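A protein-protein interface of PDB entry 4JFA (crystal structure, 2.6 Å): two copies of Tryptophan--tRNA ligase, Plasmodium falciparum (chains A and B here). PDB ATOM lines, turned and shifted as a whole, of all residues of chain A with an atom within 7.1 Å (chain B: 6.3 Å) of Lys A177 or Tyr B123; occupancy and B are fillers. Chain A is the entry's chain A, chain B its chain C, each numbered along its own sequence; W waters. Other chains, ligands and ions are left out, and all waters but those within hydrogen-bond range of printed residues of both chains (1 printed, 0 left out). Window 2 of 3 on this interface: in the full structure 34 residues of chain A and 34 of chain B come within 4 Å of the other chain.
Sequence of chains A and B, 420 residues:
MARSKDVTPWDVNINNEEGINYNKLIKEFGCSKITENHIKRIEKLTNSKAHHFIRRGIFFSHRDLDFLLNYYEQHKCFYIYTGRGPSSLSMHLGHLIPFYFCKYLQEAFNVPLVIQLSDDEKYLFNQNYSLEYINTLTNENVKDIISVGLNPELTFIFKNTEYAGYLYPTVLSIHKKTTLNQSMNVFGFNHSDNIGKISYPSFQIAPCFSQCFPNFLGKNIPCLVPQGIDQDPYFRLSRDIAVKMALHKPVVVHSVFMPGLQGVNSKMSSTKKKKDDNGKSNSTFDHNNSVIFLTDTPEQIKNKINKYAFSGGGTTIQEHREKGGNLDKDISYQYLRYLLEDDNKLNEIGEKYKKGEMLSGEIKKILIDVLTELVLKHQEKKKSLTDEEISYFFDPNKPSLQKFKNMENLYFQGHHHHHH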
ATOM      1  N   PRO A 169     -26.721 -18.805  31.978  1.00  0.00           N
ATOM      2  CA  PRO A 169     -25.954 -19.955  31.480  1.00  0.00           C
ATOM      3  C   PRO A 169     -26.713 -21.278  31.605  1.00  0.00           C
ATOM      4  O   PRO A 169     -26.598 -22.128  30.719  1.00  0.00           O
ATOM      5  CB  PRO A 169     -24.721 -19.971  32.388  1.00  0.00           C
ATOM      6  CG  PRO A 169     -24.554 -18.550  32.816  1.00  0.00           C
ATOM      7  CD  PRO A 169     -25.960 -18.034  32.982  1.00  0.00           C
ATOM      8  N   THR A 170     -27.478 -21.445  32.682  1.00  0.00           N
ATOM      9  CA  THR A 170     -28.274 -22.655  32.869  1.00  0.00           C
ATOM     10  C   THR A 170     -29.461 -22.678  31.903  1.00  0.00           C
ATOM     11  O   THR A 170     -29.810 -23.732  31.361  1.00  0.00           O
ATOM     12  CB  THR A 170     -28.786 -22.785  34.314  1.00  0.00           C
ATOM     13  OG1 THR A 170     -27.708 -22.545  35.229  1.00  0.00           O
ATOM     14  CG2 THR A 170     -29.354 -24.178  34.556  1.00  0.00           C
ATOM     15  N   VAL A 171     -30.076 -21.516  31.698  1.00  0.00           N
ATOM     16  CA  VAL A 171     -31.192 -21.382  30.764  1.00  0.00           C
ATOM     17  C   VAL A 171     -30.746 -21.725  29.342  1.00  0.00           C
ATOM     18  O   VAL A 171     -31.489 -22.351  28.584  1.00  0.00           O
ATOM     19  CB  VAL A 171     -31.788 -19.959  30.815  1.00  0.00           C
ATOM     20  CG1 VAL A 171     -32.701 -19.701  29.626  1.00  0.00           C
ATOM     21  CG2 VAL A 171     -32.544 -19.750  32.119  1.00  0.00           C
ATOM     22  N   LEU A 172     -29.524 -21.324  28.999  1.00  0.00           N
ATOM     23  CA  LEU A 172     -28.945 -21.607  27.688  1.00  0.00           C
ATOM     24  C   LEU A 172     -28.827 -23.108  27.429  1.00  0.00           C
ATOM     25  O   LEU A 172     -29.128 -23.580  26.331  1.00  0.00           O
ATOM     26  CB  LEU A 172     -27.570 -20.947  27.562  1.00  0.00           C
ATOM     27  CG  LEU A 172     -27.540 -19.436  27.320  1.00  0.00           C
ATOM     28  CD1 LEU A 172     -26.127 -18.893  27.469  1.00  0.00           C
ATOM     29  CD2 LEU A 172     -28.084 -19.114  25.941  1.00  0.00           C
ATOM     30  N   SER A 173     -28.392 -23.854  28.441  1.00  0.00           N
ATOM     31  CA  SER A 173     -28.270 -25.303  28.330  1.00  0.00           C
ATOM     32  C   SER A 173     -29.645 -25.943  28.173  1.00  0.00           C
ATOM     33  O   SER A 173     -29.819 -26.881  27.392  1.00  0.00           O
ATOM     34  CB  SER A 173     -27.561 -25.868  29.562  1.00  0.00           C
ATOM     35  OG  SER A 173     -27.469 -27.279  29.497  1.00  0.00           O
ATOM     36  N   ILE A 174     -30.618 -25.423  28.917  1.00  0.00           N
ATOM     37  CA  ILE A 174     -31.993 -25.903  28.847  1.00  0.00           C
ATOM     38  C   ILE A 174     -32.613 -25.551  27.496  1.00  0.00           C
ATOM     39  O   ILE A 174     -33.330 -26.361  26.901  1.00  0.00           O
ATOM     40  CB  ILE A 174     -32.838 -25.310  29.991  1.00  0.00           C
ATOM     41  CG1 ILE A 174     -32.269 -25.741  31.346  1.00  0.00           C
ATOM     42  CG2 ILE A 174     -34.285 -25.744  29.873  1.00  0.00           C
ATOM     43  CD1 ILE A 174     -32.853 -24.993  32.523  1.00  0.00           C
ATOM     44  N   HIS A 175     -32.336 -24.340  27.022  1.00  0.00           N
ATOM     45  CA  HIS A 175     -32.765 -23.899  25.698  1.00  0.00           C
ATOM     46  C   HIS A 175     -32.285 -24.874  24.632  1.00  0.00           C
ATOM     47  O   HIS A 175     -33.073 -25.384  23.835  1.00  0.00           O
ATOM     48  CB  HIS A 175     -32.188 -22.516  25.394  1.00  0.00           C
ATOM     49  CG  HIS A 175     -33.038 -21.379  25.870  1.00  0.00           C
ATOM     50  ND1 HIS A 175     -34.281 -21.558  26.434  1.00  0.00           N
ATOM     51  CD2 HIS A 175     -32.820 -20.042  25.853  1.00  0.00           C
ATOM     52  CE1 HIS A 175     -34.792 -20.380  26.750  1.00  0.00           C
ATOM     53  NE2 HIS A 175     -33.927 -19.446  26.409  1.00  0.00           N
ATOM     54  N   LYS A 176     -30.979 -25.123  24.637  1.00  0.00           N
ATOM     55  CA  LYS A 176     -30.311 -25.940  23.630  1.00  0.00           C
ATOM     56  C   LYS A 176     -30.835 -27.376  23.598  1.00  0.00           C
ATOM     57  O   LYS A 176     -30.727 -28.066  22.581  1.00  0.00           O
ATOM     58  CB  LYS A 176     -28.804 -25.931  23.899  1.00  0.00           C
ATOM     59  CG  LYS A 176     -27.947 -26.551  22.807  1.00  0.00           C
ATOM     60  CD  LYS A 176     -26.469 -26.344  23.113  1.00  0.00           C
ATOM     61  CE  LYS A 176     -25.589 -27.038  22.085  1.00  0.00           C
ATOM     62  NZ  LYS A 176     -24.145 -26.768  22.330  1.00  0.00           N
ATOM     63  N   LYS A 177     -31.419 -27.815  24.710  1.00  0.00           N
ATOM     64  CA  LYS A 177     -31.925 -29.178  24.825  1.00  0.00           C
ATOM     65  C   LYS A 177     -33.435 -29.248  24.631  1.00  0.00           C
ATOM     66  O   LYS A 177     -34.047 -30.300  24.833  1.00  0.00           O
ATOM     67  CB  LYS A 177     -31.532 -29.772  26.178  1.00  0.00           C
ATOM     68  CG  LYS A 177     -30.030 -29.905  26.357  1.00  0.00           C
ATOM     69  CD  LYS A 177     -29.663 -30.328  27.766  1.00  0.00           C
ATOM     70  CE  LYS A 177     -28.164 -30.548  27.877  1.00  0.00           C
ATOM     71  NZ  LYS A 177     -27.398 -29.357  27.420  1.00  0.00           N
ATOM     72  N   THR A 178     -34.030 -28.127  24.235  1.00  0.00           N
ATOM     73  CA  THR A 178     -35.460 -28.087  23.951  1.00  0.00           C
ATOM     74  C   THR A 178     -35.703 -27.646  22.511  1.00  0.00           C
ATOM     75  O   THR A 178     -35.374 -26.517  22.138  1.00  0.00           O
ATOM     76  CB  THR A 178     -36.197 -27.118  24.892  1.00  0.00           C
ATOM     77  OG1 THR A 178     -35.808 -27.368  26.249  1.00  0.00           O
ATOM     78  CG2 THR A 178     -37.703 -27.283  24.752  1.00  0.00           C
ATOM     79  N   THR A 179     -36.275 -28.529  21.700  1.00  0.00           N
ATOM     80  CA  THR A 179     -36.622 -28.167  20.330  1.00  0.00           C
ATOM     81  C   THR A 179     -37.911 -27.353  20.324  1.00  0.00           C
ATOM     82  O   THR A 179     -38.771 -27.541  21.189  1.00  0.00           O
ATOM     83  CB  THR A 179     -36.775 -29.407  19.425  1.00  0.00           C
ATOM     84  OG1 THR A 179     -37.858 -30.222  19.891  1.00  0.00           O
ATOM     85  CG2 THR A 179     -35.492 -30.225  19.422  1.00  0.00           C
ATOM     86  N   GLN A 182     -40.978 -29.361  20.483  1.00  0.00           N
ATOM     87  CA  GLN A 182     -41.240 -29.855  21.830  1.00  0.00           C
ATOM     88  C   GLN A 182     -41.876 -28.780  22.705  1.00  0.00           C
ATOM     89  O   GLN A 182     -42.827 -29.051  23.432  1.00  0.00           O
ATOM     90  CB  GLN A 182     -39.947 -30.364  22.473  1.00  0.00           C
ATOM     91  CG  GLN A 182     -40.150 -31.081  23.800  1.00  0.00           C
ATOM     92  CD  GLN A 182     -38.873 -31.713  24.325  1.00  0.00           C
ATOM     93  OE1 GLN A 182     -37.768 -31.298  23.970  1.00  0.00           O
ATOM     94  NE2 GLN A 182     -39.020 -32.724  25.173  1.00  0.00           N
ATOM     95  N   LEU A 237     -40.796 -31.642  32.075  1.00  0.00           N
ATOM     96  CA  LEU A 237     -39.771 -31.301  31.096  1.00  0.00           C
ATOM     97  C   LEU A 237     -38.422 -31.070  31.772  1.00  0.00           C
ATOM     98  O   LEU A 237     -37.374 -31.348  31.190  1.00  0.00           O
ATOM     99  CB  LEU A 237     -40.187 -30.051  30.316  1.00  0.00           C
ATOM    100  CG  LEU A 237     -39.253 -29.568  29.205  1.00  0.00           C
ATOM    101  CD1 LEU A 237     -39.155 -30.609  28.105  1.00  0.00           C
ATOM    102  CD2 LEU A 237     -39.722 -28.234  28.638  1.00  0.00           C
ATOM    103  N   ASP A 240     -36.603 -34.513  32.315  1.00  0.00           N
ATOM    104  CA  ASP A 240     -36.002 -35.098  31.119  1.00  0.00           C
ATOM    105  C   ASP A 240     -34.729 -34.347  30.734  1.00  0.00           C
ATOM    106  O   ASP A 240     -33.799 -34.925  30.169  1.00  0.00           O
ATOM    107  CB  ASP A 240     -36.988 -35.079  29.948  1.00  0.00           C
ATOM    108  CG  ASP A 240     -38.308 -35.751  30.281  1.00  0.00           C
ATOM    109  OD1 ASP A 240     -38.396 -36.416  31.335  1.00  0.00           O
ATOM    110  OD2 ASP A 240     -39.256 -35.621  29.477  1.00  0.00           O
ATOM    111  N   ILE A 241     -34.697 -33.054  31.047  1.00  0.00           N
ATOM    112  CA  ILE A 241     -33.563 -32.196  30.711  1.00  0.00           C
ATOM    113  C   ILE A 241     -32.409 -32.363  31.706  1.00  0.00           C
ATOM    114  O   ILE A 241     -31.239 -32.313  31.322  1.00  0.00           O
ATOM    115  CB  ILE A 241     -34.002 -30.714  30.593  1.00  0.00           C
ATOM    116  CG1 ILE A 241     -34.847 -30.527  29.331  1.00  0.00           C
ATOM    117  CG2 ILE A 241     -32.805 -29.780  30.562  1.00  0.00           C
ATOM    118  CD1 ILE A 241     -35.303 -29.108  29.095  1.00  0.00           C
ATOM    119  N   ALA A 242     -32.744 -32.583  32.976  1.00  0.00           N
ATOM    120  CA  ALA A 242     -31.739 -32.854  34.003  1.00  0.00           C
ATOM    121  C   ALA A 242     -30.887 -34.064  33.626  1.00  0.00           C
ATOM    122  O   ALA A 242     -29.662 -34.041  33.769  1.00  0.00           O
ATOM    123  CB  ALA A 242     -32.406 -33.076  35.348  1.00  0.00           C
ATOM    124  N   VAL A 243     -31.551 -35.114  33.144  1.00  0.00           N
ATOM    125  CA  VAL A 243     -30.884 -36.324  32.667  1.00  0.00           C
ATOM    126  C   VAL A 243     -29.851 -35.993  31.590  1.00  0.00           C
ATOM    127  O   VAL A 243     -28.780 -36.602  31.534  1.00  0.00           O
ATOM    128  CB  VAL A 243     -31.914 -37.331  32.109  1.00  0.00           C
ATOM    129  CG1 VAL A 243     -31.226 -38.569  31.564  1.00  0.00           C
ATOM    130  CG2 VAL A 243     -32.915 -37.718  33.188  1.00  0.00           C
ATOM    131  N   LYS A 244     -30.171 -35.012  30.749  1.00  0.00           N
ATOM    132  CA  LYS A 244     -29.269 -34.584  29.684  1.00  0.00           C
ATOM    133  C   LYS A 244     -28.140 -33.702  30.209  1.00  0.00           C
ATOM    134  O   LYS A 244     -27.065 -33.641  29.613  1.00  0.00           O
ATOM    135  CB  LYS A 244     -30.047 -33.841  28.597  1.00  0.00           C
ATOM    136  CG  LYS A 244     -31.114 -34.680  27.906  1.00  0.00           C
ATOM    137  CD  LYS A 244     -31.801 -33.888  26.800  1.00  0.00           C
ATOM    138  CE  LYS A 244     -32.848 -34.730  26.088  1.00  0.00           C
ATOM    139  NZ  LYS A 244     -33.501 -33.983  24.976  1.00  0.00           N
ATOM    140  N   MET A 245     -28.388 -33.017  31.321  1.00  0.00           N
ATOM    141  CA  MET A 245     -27.379 -32.151  31.925  1.00  0.00           C
ATOM    142  C   MET A 245     -26.621 -32.891  33.018  1.00  0.00           C
ATOM    143  O   MET A 245     -25.735 -32.323  33.660  1.00  0.00           O
ATOM    144  CB  MET A 245     -28.026 -30.894  32.511  1.00  0.00           C
ATOM    145  CG  MET A 245     -28.851 -30.097  31.519  1.00  0.00           C
ATOM    146  SD  MET A 245     -29.575 -28.622  32.264  1.00  0.00           S
ATOM    147  CE  MET A 245     -28.089 -27.737  32.743  1.00  0.00           C
ATOM    148  N   ALA A 246     -26.984 -34.158  33.219  1.00  0.00           N
ATOM    149  CA  ALA A 246     -26.396 -35.004  34.260  1.00  0.00           C
ATOM    150  C   ALA A 246     -26.596 -34.426  35.661  1.00  0.00           C
ATOM    151  O   ALA A 246     -25.756 -34.611  36.544  1.00  0.00           O
ATOM    152  CB  ALA A 246     -24.917 -35.256  33.986  1.00  0.00           C
ATOM    153  N   SER B 118     -21.366 -12.807  21.157  1.00  0.00           N
ATOM    154  CA  SER B 118     -22.482 -13.735  21.200  1.00  0.00           C
ATOM    155  C   SER B 118     -22.026 -15.165  21.449  1.00  0.00           C
ATOM    156  O   SER B 118     -22.214 -16.047  20.602  1.00  0.00           O
ATOM    157  CB  SER B 118     -23.267 -13.653  19.893  1.00  0.00           C
ATOM    158  OG  SER B 118     -22.400 -13.631  18.771  1.00  0.00           O
ATOM    159  N   ASP B 119     -21.433 -15.389  22.617  1.00  0.00           N
ATOM    160  CA  ASP B 119     -21.024 -16.724  23.024  1.00  0.00           C
ATOM    161  C   ASP B 119     -22.244 -17.615  23.211  1.00  0.00           C
ATOM    162  O   ASP B 119     -22.190 -18.826  22.969  1.00  0.00           O
ATOM    163  CB  ASP B 119     -20.188 -16.657  24.302  1.00  0.00           C
ATOM    164  CG  ASP B 119     -20.783 -15.730  25.344  1.00  0.00           C
ATOM    165  OD1 ASP B 119     -21.806 -15.078  25.053  1.00  0.00           O
ATOM    166  OD2 ASP B 119     -20.217 -15.637  26.454  1.00  0.00           O
ATOM    167  N   ASP B 120     -23.348 -17.003  23.630  1.00  0.00           N
ATOM    168  CA  ASP B 120     -24.613 -17.711  23.762  1.00  0.00           C
ATOM    169  C   ASP B 120     -25.104 -18.214  22.404  1.00  0.00           C
ATOM    170  O   ASP B 120     -25.536 -19.359  22.280  1.00  0.00           O
ATOM    171  CB  ASP B 120     -25.663 -16.815  24.425  1.00  0.00           C
ATOM    172  CG  ASP B 120     -25.867 -15.507  23.685  1.00  0.00           C
ATOM    173  OD1 ASP B 120     -25.039 -15.177  22.810  1.00  0.00           O
ATOM    174  OD2 ASP B 120     -26.852 -14.802  23.982  1.00  0.00           O
ATOM    175  N   GLU B 121     -25.023 -17.355  21.390  1.00  0.00           N
ATOM    176  CA  GLU B 121     -25.423 -17.720  20.037  1.00  0.00           C
ATOM    177  C   GLU B 121     -24.609 -18.902  19.540  1.00  0.00           C
ATOM    178  O   GLU B 121     -25.164 -19.892  19.070  1.00  0.00           O
ATOM    179  CB  GLU B 121     -25.231 -16.541  19.083  1.00  0.00           C
ATOM    180  CG  GLU B 121     -25.536 -16.868  17.623  1.00  0.00           C
ATOM    181  CD  GLU B 121     -24.892 -15.892  16.652  1.00  0.00           C
ATOM    182  OE1 GLU B 121     -24.063 -15.064  17.090  1.00  0.00           O
ATOM    183  OE2 GLU B 121     -25.209 -15.958  15.446  1.00  0.00           O
ATOM    184  N   LYS B 122     -23.290 -18.793  19.640  1.00  0.00           N
ATOM    185  CA  LYS B 122     -22.406 -19.849  19.161  1.00  0.00           C
ATOM    186  C   LYS B 122     -22.530 -21.135  19.971  1.00  0.00           C
ATOM    187  O   LYS B 122     -22.245 -22.223  19.465  1.00  0.00           O
ATOM    188  CB  LYS B 122     -20.958 -19.361  19.119  1.00  0.00           C
ATOM    189  CG  LYS B 122     -20.739 -18.213  18.138  1.00  0.00           C
ATOM    190  CD  LYS B 122     -21.389 -18.539  16.797  1.00  0.00           C
ATOM    191  CE  LYS B 122     -21.462 -17.315  15.898  1.00  0.00           C
ATOM    192  NZ  LYS B 122     -22.175 -17.622  14.624  1.00  0.00           N
ATOM    193  N   TYR B 123     -22.968 -21.012  21.220  1.00  0.00           N
ATOM    194  CA  TYR B 123     -23.249 -22.189  22.029  1.00  0.00           C
ATOM    195  C   TYR B 123     -24.541 -22.859  21.581  1.00  0.00           C
ATOM    196  O   TYR B 123     -24.645 -24.085  21.585  1.00  0.00           O
ATOM    197  CB  TYR B 123     -23.340 -21.831  23.515  1.00  0.00           C
ATOM    198  CG  TYR B 123     -23.841 -22.971  24.372  1.00  0.00           C
ATOM    199  CD1 TYR B 123     -23.118 -24.149  24.481  1.00  0.00           C
ATOM    200  CD2 TYR B 123     -25.036 -22.870  25.071  1.00  0.00           C
ATOM    201  CE1 TYR B 123     -23.570 -25.197  25.258  1.00  0.00           C
ATOM    202  CE2 TYR B 123     -25.496 -23.917  25.855  1.00  0.00           C
ATOM    203  CZ  TYR B 123     -24.757 -25.075  25.943  1.00  0.00           C
ATOM    204  OH  TYR B 123     -25.204 -26.118  26.717  1.00  0.00           O
ATOM    205  N   LEU B 124     -25.521 -22.048  21.197  1.00  0.00           N
ATOM    206  CA  LEU B 124     -26.844 -22.544  20.828  1.00  0.00           C
ATOM    207  C   LEU B 124     -26.907 -23.114  19.411  1.00  0.00           C
ATOM    208  O   LEU B 124     -27.693 -24.025  19.136  1.00  0.00           O
ATOM    209  CB  LEU B 124     -27.884 -21.431  20.988  1.00  0.00           C
ATOM    210  CG  LEU B 124     -28.197 -20.978  22.416  1.00  0.00           C
ATOM    211  CD1 LEU B 124     -28.920 -19.637  22.411  1.00  0.00           C
ATOM    212  CD2 LEU B 124     -29.022 -22.030  23.137  1.00  0.00           C
ATOM    213  N   PHE B 125     -26.084 -22.576  18.517  1.00  0.00           N
ATOM    214  CA  PHE B 125     -26.120 -22.953  17.108  1.00  0.00           C
ATOM    215  C   PHE B 125     -25.145 -24.081  16.780  1.00  0.00           C
ATOM    216  O   PHE B 125     -25.261 -24.723  15.736  1.00  0.00           O
ATOM    217  CB  PHE B 125     -25.843 -21.734  16.222  1.00  0.00           C
ATOM    218  CG  PHE B 125     -27.027 -20.820  16.057  1.00  0.00           C
ATOM    219  CD1 PHE B 125     -27.786 -20.851  14.896  1.00  0.00           C
ATOM    220  CD2 PHE B 125     -27.385 -19.929  17.059  1.00  0.00           C
ATOM    221  CE1 PHE B 125     -28.877 -20.012  14.741  1.00  0.00           C
ATOM    222  CE2 PHE B 125     -28.475 -19.089  16.909  1.00  0.00           C
ATOM    223  CZ  PHE B 125     -29.221 -19.131  15.749  1.00  0.00           C
ATOM    224  N   ASN B 126     -24.184 -24.314  17.668  1.00  0.00           N
ATOM    225  CA  ASN B 126     -23.237 -25.411  17.485  1.00  0.00           C
ATOM    226  C   ASN B 126     -23.503 -26.567  18.452  1.00  0.00           C
ATOM    227  O   ASN B 126     -23.157 -26.498  19.632  1.00  0.00           O
ATOM    228  CB  ASN B 126     -21.796 -24.906  17.596  1.00  0.00           C
ATOM    229  CG  ASN B 126     -21.400 -24.013  16.431  1.00  0.00           C
ATOM    230  OD1 ASN B 126     -21.186 -24.489  15.314  1.00  0.00           O
ATOM    231  ND2 ASN B 126     -21.299 -22.715  16.685  1.00  0.00           N
ATOM    232  N   GLN B 127     -24.113 -27.628  17.927  1.00  0.00           N
ATOM    233  CA  GLN B 127     -24.641 -28.734  18.730  1.00  0.00           C
ATOM    234  C   GLN B 127     -23.640 -29.395  19.681  1.00  0.00           C
ATOM    235  O   GLN B 127     -23.971 -29.695  20.832  1.00  0.00           O
ATOM    236  CB  GLN B 127     -25.255 -29.795  17.810  1.00  0.00           C
ATOM    237  CG  GLN B 127     -25.932 -30.942  18.544  1.00  0.00           C
ATOM    238  CD  GLN B 127     -27.090 -30.477  19.406  1.00  0.00           C
ATOM    239  OE1 GLN B 127     -27.804 -29.537  19.053  1.00  0.00           O
ATOM    240  NE2 GLN B 127     -27.280 -31.131  20.546  1.00  0.00           N
ATOM    241  N   TYR B 129     -20.689 -28.158  20.696  1.00  0.00           N
ATOM    242  CA  TYR B 129     -19.852 -27.209  21.425  1.00  0.00           C
ATOM    243  C   TYR B 129     -20.376 -26.981  22.842  1.00  0.00           C
ATOM    244  O   TYR B 129     -21.584 -26.826  23.048  1.00  0.00           O
ATOM    245  CB  TYR B 129     -19.766 -25.869  20.684  1.00  0.00           C
ATOM    246  CG  TYR B 129     -18.859 -25.874  19.470  1.00  0.00           C
ATOM    247  CD1 TYR B 129     -18.579 -24.697  18.786  1.00  0.00           C
ATOM    248  CD2 TYR B 129     -18.287 -27.052  19.003  1.00  0.00           C
ATOM    249  CE1 TYR B 129     -17.755 -24.692  17.675  1.00  0.00           C
ATOM    250  CE2 TYR B 129     -17.463 -27.054  17.894  1.00  0.00           C
ATOM    251  CZ  TYR B 129     -17.200 -25.873  17.235  1.00  0.00           C
ATOM    252  OH  TYR B 129     -16.379 -25.879  16.131  1.00  0.00           O
ATOM    253  N   SER B 130     -19.468 -26.968  23.815  1.00  0.00           N
ATOM    254  CA  SER B 130     -19.828 -26.646  25.192  1.00  0.00           C
ATOM    255  C   SER B 130     -19.547 -25.175  25.465  1.00  0.00           C
ATOM    256  O   SER B 130     -18.909 -24.500  24.656  1.00  0.00           O
ATOM    257  CB  SER B 130     -19.038 -27.510  26.174  1.00  0.00           C
ATOM    258  OG  SER B 130     -17.664 -27.162  26.167  1.00  0.00           O
ATOM    259  N   LEU B 131     -20.019 -24.681  26.607  1.00  0.00           N
ATOM    260  CA  LEU B 131     -19.824 -23.282  26.982  1.00  0.00           C
ATOM    261  C   LEU B 131     -18.362 -22.931  27.267  1.00  0.00           C
ATOM    262  O   LEU B 131     -17.917 -21.823  26.956  1.00  0.00           O
ATOM    263  CB  LEU B 131     -20.700 -22.925  28.185  1.00  0.00           C
ATOM    264  CG  LEU B 131     -22.164 -22.606  27.876  1.00  0.00           C
ATOM    265  CD1 LEU B 131     -23.017 -22.689  29.132  1.00  0.00           C
ATOM    266  CD2 LEU B 131     -22.274 -21.225  27.255  1.00  0.00           C
ATOM    267  N   ILE B 134     -16.537 -22.602  23.818  1.00  0.00           N
ATOM    268  CA  ILE B 134     -16.980 -21.321  23.294  1.00  0.00           C
ATOM    269  C   ILE B 134     -16.289 -20.172  24.024  1.00  0.00           C
ATOM    270  O   ILE B 134     -15.966 -19.161  23.416  1.00  0.00           O
ATOM    271  CB  ILE B 134     -18.514 -21.167  23.409  1.00  0.00           C
ATOM    272  CG1 ILE B 134     -19.225 -22.170  22.496  1.00  0.00           C
ATOM    273  CG2 ILE B 134     -18.948 -19.760  23.045  1.00  0.00           C
ATOM    274  CD1 ILE B 134     -18.986 -21.932  21.016  1.00  0.00           C
ATOM    275  N   ASN B 194     -33.536 -25.469  18.279  1.00  0.00           N
ATOM    276  CA  ASN B 194     -33.815 -25.240  19.694  1.00  0.00           C
ATOM    277  C   ASN B 194     -34.309 -23.819  19.956  1.00  0.00           C
ATOM    278  O   ASN B 194     -33.996 -22.890  19.207  1.00  0.00           O
ATOM    279  CB  ASN B 194     -32.603 -25.574  20.570  1.00  0.00           C
ATOM    280  CG  ASN B 194     -31.422 -24.655  20.319  1.00  0.00           C
ATOM    281  OD1 ASN B 194     -31.393 -23.520  20.794  1.00  0.00           O
ATOM    282  ND2 ASN B 194     -30.428 -25.151  19.593  1.00  0.00           N
HETATM  283  O   HOH W   1     -24.096 -28.984  24.223  1.00  0.00           O
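NZ of Lys A176 is in hydrogen-bond range of O of Tyr B123. The side-chain amino group (NZ) of Lys A176 sits at hydrogen-bond distance from the backbone carbonyl oxygen (O) of Asn B126 (2.9 Å). The side-chain amino group (NZ) of Lys A176 sits at hydrogen-bond distance from the backbone carbonyl oxygen (O) of Gln B127 (3.3 Å). NZ of Lys A176 sits at hydrogen-bond distance from O of Tyr B129 (2.7 Å).
The side-chain hydroxyl of Ser A173 sits at hydrogen-bond distance from the side-chain amino group of Lys A177. OG of Ser A173 sits close to SD of Met A245 (3.7 Å). O of Ile A174 lies within hydrogen-bond range of OG1 of Thr A178 (2.8 Å). The backbone carbonyl oxygen (O) of Lys B122 lies within hydrogen-bond range of the side-chain amide nitrogen (ND2) of Asn B126 (3.0 Å). The backbone carbonyl oxygen of Leu B124 lies within hydrogen-bond range of the side-chain amide nitrogen of Asn B194 (3.0 Å).
No position is printed for both chains.
Water W1 bridges NZ of Lys A176 (2.9 Å) and O of Gln B127 (3.5 Å).
Of the printed residues of chain B, Thr A178 touches Asn B194. Of chain A, only Leu A172, Ser A173, Lys A176 and Lys A177 come within 4 Å of Tyr B123. Printed residues of chain A within 4 Å of Leu B124: Leu A172 (3.6 Å), His A175 (3.9 Å) and Lys A176 (3.96 Å). Printed residues of chain A within 4 Å of Tyr B129: Lys A176 (2.7 Å). Printed residues of chain A within 4 Å of Leu B131: Pro A169 (3.96 Å).
Pro A169 touches Leu B131. CD2 of Leu A172 touches CB of Asp B120 (3.7 Å). CD2 of Leu B124 touches O of Leu A172 (3.6 Å). Tyr B123 touches Ser A173. CB of His A175 touches CD2 of Leu B124, at 3.9 Å. His A175 touches Asn B194 (O to CB, 3.3 Å). N of Lys A176 touches CD2 of Leu B124 (3.96 Å). Asn B194 touches Lys A176. OH of Tyr B123 touches NZ of Lys A177, at 3.97 Å. O of Thr A178 touches CA of Asn B194 (3.2 Å).
Hydrophobic or aromatic side chains of chain B within 4 Å of the printed part of chain A: Tyr B123, Leu B124 and Leu B131. Hydrophobic or aromatic side chains of chain A within 4 Å of the printed part of chain B: Leu A172 and His A175.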
